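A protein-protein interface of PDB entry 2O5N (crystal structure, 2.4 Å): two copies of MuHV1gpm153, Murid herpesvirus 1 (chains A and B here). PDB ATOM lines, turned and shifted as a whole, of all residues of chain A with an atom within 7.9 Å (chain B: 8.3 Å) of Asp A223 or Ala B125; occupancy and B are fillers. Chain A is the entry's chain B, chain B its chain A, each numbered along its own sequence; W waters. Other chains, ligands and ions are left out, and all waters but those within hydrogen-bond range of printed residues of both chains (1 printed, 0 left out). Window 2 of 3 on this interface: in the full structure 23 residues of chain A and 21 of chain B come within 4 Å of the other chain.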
ATOM      1  N   TRP A 218     -13.334 -12.654  31.164  1.00  0.00           N
ATOM      2  CA  TRP A 218     -12.863 -12.546  29.782  1.00  0.00           C
ATOM      3  C   TRP A 218     -11.887 -11.388  29.618  1.00  0.00           C
ATOM      4  O   TRP A 218     -12.074 -10.320  30.207  1.00  0.00           O
ATOM      5  CB  TRP A 218     -14.039 -12.271  28.827  1.00  0.00           C
ATOM      6  CG  TRP A 218     -15.005 -13.374  28.582  1.00  0.00           C
ATOM      7  CD1 TRP A 218     -16.193 -13.569  29.219  1.00  0.00           C
ATOM      8  CD2 TRP A 218     -14.903 -14.422  27.593  1.00  0.00           C
ATOM      9  NE1 TRP A 218     -16.831 -14.681  28.702  1.00  0.00           N
ATOM     10  CE2 TRP A 218     -16.059 -15.224  27.713  1.00  0.00           C
ATOM     11  CE3 TRP A 218     -13.934 -14.770  26.639  1.00  0.00           C
ATOM     12  CZ2 TRP A 218     -16.295 -16.329  26.893  1.00  0.00           C
ATOM     13  CZ3 TRP A 218     -14.166 -15.882  25.824  1.00  0.00           C
ATOM     14  CH2 TRP A 218     -15.342 -16.644  25.958  1.00  0.00           C
ATOM     15  N   SER A 219     -10.864 -11.581  28.786  1.00  0.00           N
ATOM     16  CA  SER A 219      -9.997 -10.465  28.379  1.00  0.00           C
ATOM     17  C   SER A 219     -10.736  -9.519  27.426  1.00  0.00           C
ATOM     18  O   SER A 219     -11.823  -9.845  26.939  1.00  0.00           O
ATOM     19  CB  SER A 219      -8.711 -10.976  27.738  1.00  0.00           C
ATOM     20  OG  SER A 219      -9.007 -11.792  26.628  1.00  0.00           O
ATOM     21  N   ALA A 220     -10.159  -8.345  27.185  1.00  0.00           N
ATOM     22  CA  ALA A 220     -10.743  -7.331  26.288  1.00  0.00           C
ATOM     23  C   ALA A 220     -11.088  -7.916  24.917  1.00  0.00           C
ATOM     24  O   ALA A 220     -12.235  -7.808  24.471  1.00  0.00           O
ATOM     25  CB  ALA A 220      -9.821  -6.141  26.157  1.00  0.00           C
ATOM     26  N   GLY A 221     -10.109  -8.535  24.253  1.00  0.00           N
ATOM     27  CA  GLY A 221     -10.406  -9.508  23.195  1.00  0.00           C
ATOM     28  C   GLY A 221     -11.023 -10.708  23.903  1.00  0.00           C
ATOM     29  O   GLY A 221     -10.576 -11.103  24.989  1.00  0.00           O
ATOM     30  N   ARG A 222     -12.066 -11.297  23.342  1.00  0.00           N
ATOM     31  CA  ARG A 222     -12.639 -12.457  24.007  1.00  0.00           C
ATOM     32  C   ARG A 222     -11.841 -13.671  23.574  1.00  0.00           C
ATOM     33  O   ARG A 222     -12.380 -14.594  22.948  1.00  0.00           O
ATOM     34  CB  ARG A 222     -14.116 -12.608  23.660  1.00  0.00           C
ATOM     35  CG  ARG A 222     -14.917 -11.334  23.839  1.00  0.00           C
ATOM     36  CD  ARG A 222     -16.393 -11.647  24.019  1.00  0.00           C
ATOM     37  NE  ARG A 222     -16.812 -11.457  25.398  1.00  0.00           N
ATOM     38  CZ  ARG A 222     -17.805 -12.123  25.986  1.00  0.00           C
ATOM     39  NH1 ARG A 222     -18.489 -13.061  25.325  1.00  0.00           N
ATOM     40  NH2 ARG A 222     -18.108 -11.857  27.247  1.00  0.00           N
ATOM     41  N   ASP A 223     -10.546 -13.643  23.884  1.00  0.00           N
ATOM     42  CA  ASP A 223      -9.595 -14.625  23.374  1.00  0.00           C
ATOM     43  C   ASP A 223      -8.848 -15.314  24.518  1.00  0.00           C
ATOM     44  O   ASP A 223      -8.044 -16.228  24.319  1.00  0.00           O
ATOM     45  CB  ASP A 223      -8.616 -13.966  22.385  1.00  0.00           C
ATOM     46  CG  ASP A 223      -7.748 -12.892  23.024  1.00  0.00           C
ATOM     47  OD1 ASP A 223      -8.161 -12.253  24.015  1.00  0.00           O
ATOM     48  OD2 ASP A 223      -6.635 -12.662  22.519  1.00  0.00           O
ATOM     49  N   SER A 224      -9.138 -14.865  25.721  1.00  0.00           N
ATOM     50  CA  SER A 224      -8.568 -15.432  26.911  1.00  0.00           C
ATOM     51  C   SER A 224      -9.645 -15.379  27.991  1.00  0.00           C
ATOM     52  O   SER A 224     -10.368 -14.383  28.105  1.00  0.00           O
ATOM     53  CB  SER A 224      -7.335 -14.626  27.315  1.00  0.00           C
ATOM     54  OG  SER A 224      -6.444 -15.436  28.053  1.00  0.00           O
ATOM     55  N   ARG A 225      -9.758 -16.450  28.772  1.00  0.00           N
ATOM     56  CA  ARG A 225     -10.772 -16.520  29.830  1.00  0.00           C
ATOM     57  C   ARG A 225     -10.371 -17.393  31.008  1.00  0.00           C
ATOM     58  O   ARG A 225      -9.639 -18.346  30.848  1.00  0.00           O
ATOM     59  CB  ARG A 225     -12.130 -16.986  29.272  1.00  0.00           C
ATOM     60  CG  ARG A 225     -12.159 -18.421  28.835  1.00  0.00           C
ATOM     61  CD  ARG A 225     -13.537 -18.870  28.400  1.00  0.00           C
ATOM     62  NE  ARG A 225     -13.434 -20.037  27.526  1.00  0.00           N
ATOM     63  CZ  ARG A 225     -14.454 -20.625  26.897  1.00  0.00           C
ATOM     64  NH1 ARG A 225     -15.705 -20.176  27.016  1.00  0.00           N
ATOM     65  NH2 ARG A 225     -14.215 -21.673  26.124  1.00  0.00           N
ATOM     66  N   LEU A 243      -8.002 -13.963  36.238  1.00  0.00           N
ATOM     67  CA  LEU A 243      -7.517 -13.879  34.866  1.00  0.00           C
ATOM     68  C   LEU A 243      -6.205 -13.084  34.708  1.00  0.00           C
ATOM     69  O   LEU A 243      -6.175 -11.873  34.950  1.00  0.00           O
ATOM     70  CB  LEU A 243      -8.587 -13.296  33.942  1.00  0.00           C
ATOM     71  CG  LEU A 243      -8.263 -13.306  32.448  1.00  0.00           C
ATOM     72  CD1 LEU A 243      -8.023 -14.726  31.888  1.00  0.00           C
ATOM     73  CD2 LEU A 243      -9.350 -12.599  31.695  1.00  0.00           C
ATOM     74  N   ASN A 246      -2.641  -8.743  30.164  1.00  0.00           N
ATOM     75  CA  ASN A 246      -1.656  -7.710  29.802  1.00  0.00           C
ATOM     76  C   ASN A 246      -2.145  -6.394  30.393  1.00  0.00           C
ATOM     77  O   ASN A 246      -3.271  -5.996  30.112  1.00  0.00           O
ATOM     78  CB  ASN A 246      -1.510  -7.565  28.268  1.00  0.00           C
ATOM     79  CG  ASN A 246      -0.651  -8.671  27.622  1.00  0.00           C
ATOM     80  OD1 ASN A 246       0.355  -9.123  28.178  1.00  0.00           O
ATOM     81  ND2 ASN A 246      -1.050  -9.088  26.420  1.00  0.00           N
ATOM     82  N   GLN A 249      -4.107  -3.909  28.375  1.00  0.00           N
ATOM     83  CA  GLN A 249      -5.368  -4.369  27.801  1.00  0.00           C
ATOM     84  C   GLN A 249      -6.391  -4.673  28.899  1.00  0.00           C
ATOM     85  O   GLN A 249      -7.371  -5.397  28.683  1.00  0.00           O
ATOM     86  CB  GLN A 249      -5.102  -5.585  26.916  1.00  0.00           C
ATOM     87  CG  GLN A 249      -4.223  -5.242  25.716  1.00  0.00           C
ATOM     88  CD  GLN A 249      -3.800  -6.446  24.912  1.00  0.00           C
ATOM     89  OE1 GLN A 249      -3.260  -7.419  25.453  1.00  0.00           O
ATOM     90  NE2 GLN A 249      -4.015  -6.382  23.599  1.00  0.00           N
ATOM     91  N   CYS B 108      -4.141 -27.278  15.947  1.00  0.00           N
ATOM     92  CA  CYS B 108      -4.396 -28.221  17.028  1.00  0.00           C
ATOM     93  C   CYS B 108      -5.087 -27.578  18.203  1.00  0.00           C
ATOM     94  O   CYS B 108      -4.926 -26.385  18.461  1.00  0.00           O
ATOM     95  CB  CYS B 108      -3.098 -28.904  17.514  1.00  0.00           C
ATOM     96  SG  CYS B 108      -2.107 -29.634  16.209  1.00  0.00           S
ATOM     97  N   THR B 109      -5.865 -28.397  18.899  1.00  0.00           N
ATOM     98  CA  THR B 109      -6.340 -28.091  20.234  1.00  0.00           C
ATOM     99  C   THR B 109      -5.357 -28.718  21.227  1.00  0.00           C
ATOM    100  O   THR B 109      -4.783 -29.766  20.954  1.00  0.00           O
ATOM    101  CB  THR B 109      -7.779 -28.620  20.438  1.00  0.00           C
ATOM    102  OG1 THR B 109      -8.644 -27.976  19.495  1.00  0.00           O
ATOM    103  CG2 THR B 109      -8.294 -28.320  21.848  1.00  0.00           C
ATOM    104  N   SER B 121      -6.947 -25.108  28.531  1.00  0.00           N
ATOM    105  CA  SER B 121      -7.106 -25.502  27.122  1.00  0.00           C
ATOM    106  C   SER B 121      -6.882 -24.329  26.144  1.00  0.00           C
ATOM    107  O   SER B 121      -6.915 -23.167  26.547  1.00  0.00           O
ATOM    108  CB  SER B 121      -8.461 -26.187  26.879  1.00  0.00           C
ATOM    109  OG  SER B 121      -9.541 -25.470  27.472  1.00  0.00           O
ATOM    110  N   PHE B 122      -6.656 -24.651  24.866  1.00  0.00           N
ATOM    111  CA  PHE B 122      -6.352 -23.666  23.822  1.00  0.00           C
ATOM    112  C   PHE B 122      -6.657 -24.220  22.438  1.00  0.00           C
ATOM    113  O   PHE B 122      -6.045 -25.208  22.018  1.00  0.00           O
ATOM    114  CB  PHE B 122      -4.877 -23.244  23.898  1.00  0.00           C
ATOM    115  CG  PHE B 122      -4.505 -22.105  22.978  1.00  0.00           C
ATOM    116  CD1 PHE B 122      -3.347 -22.174  22.197  1.00  0.00           C
ATOM    117  CD2 PHE B 122      -5.296 -20.957  22.891  1.00  0.00           C
ATOM    118  CE1 PHE B 122      -2.984 -21.115  21.343  1.00  0.00           C
ATOM    119  CE2 PHE B 122      -4.938 -19.890  22.044  1.00  0.00           C
ATOM    120  CZ  PHE B 122      -3.782 -19.967  21.274  1.00  0.00           C
ATOM    121  N   ASP B 123      -7.607 -23.584  21.742  1.00  0.00           N
ATOM    122  CA  ASP B 123      -7.964 -23.929  20.358  1.00  0.00           C
ATOM    123  C   ASP B 123      -7.363 -22.943  19.342  1.00  0.00           C
ATOM    124  O   ASP B 123      -7.892 -22.774  18.231  1.00  0.00           O
ATOM    125  CB  ASP B 123      -9.496 -24.016  20.192  1.00  0.00           C
ATOM    126  CG  ASP B 123     -10.217 -22.679  20.470  1.00  0.00           C
ATOM    127  OD1 ASP B 123      -9.779 -21.641  19.940  1.00  0.00           O
ATOM    128  OD2 ASP B 123     -11.237 -22.663  21.203  1.00  0.00           O
ATOM    129  N   GLY B 124      -6.275 -22.275  19.721  1.00  0.00           N
ATOM    130  CA  GLY B 124      -5.662 -21.284  18.837  1.00  0.00           C
ATOM    131  C   GLY B 124      -6.458 -19.994  18.675  1.00  0.00           C
ATOM    132  O   GLY B 124      -5.950 -19.018  18.089  1.00  0.00           O
ATOM    133  N   ALA B 125      -7.708 -19.996  19.164  1.00  0.00           N
ATOM    134  CA  ALA B 125      -8.533 -18.772  19.253  1.00  0.00           C
ATOM    135  C   ALA B 125      -8.708 -18.312  20.703  1.00  0.00           C
ATOM    136  O   ALA B 125      -8.379 -17.169  21.039  1.00  0.00           O
ATOM    137  CB  ALA B 125      -9.890 -18.967  18.578  1.00  0.00           C
ATOM    138  N   ILE B 126      -9.200 -19.210  21.560  1.00  0.00           N
ATOM    139  CA  ILE B 126      -9.436 -18.903  22.976  1.00  0.00           C
ATOM    140  C   ILE B 126      -8.557 -19.733  23.929  1.00  0.00           C
ATOM    141  O   ILE B 126      -8.561 -20.960  23.866  1.00  0.00           O
ATOM    142  CB  ILE B 126     -10.942 -19.078  23.346  1.00  0.00           C
ATOM    143  CG1 ILE B 126     -11.821 -18.212  22.434  1.00  0.00           C
ATOM    144  CG2 ILE B 126     -11.199 -18.721  24.819  1.00  0.00           C
ATOM    145  CD1 ILE B 126     -13.248 -18.701  22.305  1.00  0.00           C
ATOM    146  N   GLN B 127      -7.808 -19.056  24.800  1.00  0.00           N
ATOM    147  CA  GLN B 127      -7.162 -19.700  25.934  1.00  0.00           C
ATOM    148  C   GLN B 127      -8.178 -19.801  27.056  1.00  0.00           C
ATOM    149  O   GLN B 127      -8.892 -18.838  27.325  1.00  0.00           O
ATOM    150  CB  GLN B 127      -6.002 -18.860  26.472  1.00  0.00           C
ATOM    151  CG  GLN B 127      -4.850 -18.584  25.542  1.00  0.00           C
ATOM    152  CD  GLN B 127      -3.815 -17.710  26.192  1.00  0.00           C
ATOM    153  OE1 GLN B 127      -4.104 -16.981  27.149  1.00  0.00           O
ATOM    154  NE2 GLN B 127      -2.595 -17.781  25.695  1.00  0.00           N
ATOM    155  N   THR B 128      -8.211 -20.944  27.739  1.00  0.00           N
ATOM    156  CA  THR B 128      -9.106 -21.142  28.867  1.00  0.00           C
ATOM    157  C   THR B 128      -8.340 -21.680  30.067  1.00  0.00           C
ATOM    158  O   THR B 128      -7.584 -22.644  29.949  1.00  0.00           O
ATOM    159  CB  THR B 128     -10.272 -22.126  28.522  1.00  0.00           C
ATOM    160  OG1 THR B 128     -10.951 -21.693  27.338  1.00  0.00           O
ATOM    161  CG2 THR B 128     -11.264 -22.232  29.661  1.00  0.00           C
ATOM    162  N   ILE B 148       0.308 -22.667  28.713  1.00  0.00           N
ATOM    163  CA  ILE B 148      -1.038 -22.952  28.197  1.00  0.00           C
ATOM    164  C   ILE B 148      -1.062 -23.346  26.723  1.00  0.00           C
ATOM    165  O   ILE B 148      -1.787 -24.265  26.337  1.00  0.00           O
ATOM    166  CB  ILE B 148      -2.054 -21.780  28.499  1.00  0.00           C
ATOM    167  CG1 ILE B 148      -3.515 -22.238  28.352  1.00  0.00           C
ATOM    168  CG2 ILE B 148      -1.749 -20.536  27.658  1.00  0.00           C
ATOM    169  CD1 ILE B 148      -4.534 -21.317  29.034  1.00  0.00           C
ATOM    170  N   ARG B 149      -0.256 -22.668  25.910  1.00  0.00           N
ATOM    171  CA  ARG B 149      -0.266 -22.881  24.463  1.00  0.00           C
ATOM    172  C   ARG B 149       0.579 -24.090  24.042  1.00  0.00           C
ATOM    173  O   ARG B 149       0.493 -24.554  22.904  1.00  0.00           O
ATOM    174  CB  ARG B 149       0.160 -21.604  23.714  1.00  0.00           C
ATOM    175  CG  ARG B 149      -0.768 -20.369  23.913  1.00  0.00           C
ATOM    176  CD  ARG B 149      -0.289 -19.159  23.064  1.00  0.00           C
ATOM    177  NE  ARG B 149      -1.348 -18.183  22.777  1.00  0.00           N
ATOM    178  CZ  ARG B 149      -1.310 -17.261  21.804  1.00  0.00           C
ATOM    179  NH1 ARG B 149      -0.258 -17.168  20.989  1.00  0.00           N
ATOM    180  NH2 ARG B 149      -2.340 -16.430  21.635  1.00  0.00           N
HETATM  181  O   HOH W   1      -5.578 -16.867  22.579  1.00  0.00           O
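No position is printed for both chains.
Of the 8 pairs that touch across the chains among the printed residues, none has its exchanged pair printed and touching as well.
Of the 11 printed residues of chain A, 4 touch a printed residue of chain B.
Of the 12 printed residues of chain B, 4 touch a printed residue of chain A.
O of Ser B121 lies within hydrogen-bond range of N of Thr B128.
The side-chain carboxylate (OD1) of Asp B123 sits at hydrogen-bond distance from the backbone NH (N) of Ala B125 (2.8 Å).
The backbone NH (N) of Ile B126 is in hydrogen-bond range of the side-chain carboxylate (OD1) of Asp B123 (3.0 Å).
The side-chain amide nitrogen (NE2) of Gln B127 sits close to the guanidinium group (NE) of Arg B149 (3.2 Å).
OD1 of Asp A223 sits at hydrogen-bond distance from OG of Ser A219.
The backbone NH of Ser A219 lies within hydrogen-bond range of the backbone carbonyl oxygen of Ser A224.
Water W1 lies within hydrogen-bond range of O of Asp A223, O of Ala B125 and NH2 of Arg B149.
Of the printed residues of chain B, Asp A223 touches Ala B125 (3.4 Å), Ile B126 (3.3 Å) and Gln B127 (2.9 Å).
Ala B125 touches just one residue of chain A: Asp A223 (3.4 Å).
No residue of chain A comes within 4 Å of Gly B124.
Of the printed residues of chain B, Arg A225 touches Ile B126 (3.7 Å), Gln B127 (2.9 Å) and Thr B128 (3.0 Å).
Printed residues of chain B within 4 Å of Arg A222: Ile B126.
Printed residues of chain A within 4 Å of Ile B126: Arg A222, Asp A223 and Arg A225.
Printed residues of chain A within 4 Å of Thr B128: Arg A225 (3.0 Å).
The nearest printed residue of chain A that does not touch Thr B128 is Ser A224 (5.6 Å).
N of Gln B127 is in hydrogen-bond range of O of Asp A223 (2.9 Å).
The side-chain amide oxygen (OE1) of Gln B127 sits at hydrogen-bond distance from the side-chain hydroxyl (OG) of Ser A224 (2.9 Å).
The backbone carbonyl oxygen (O) of Gln B127 lies within hydrogen-bond range of the backbone NH (N) of Arg A225.
OG1 of Thr B128 is in hydrogen-bond range of NE of Arg A225 (3.0 Å).
O of Asp A223 sits close to O of Ala B125 (3.4 Å).
Among the printed residues, merely in contact across the chains: Arg A222 with Ile B126 (3.7 Å), Asp A223 with Ile B126 (3.3 Å) and Arg A225 with Ile B126 (3.7 Å).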
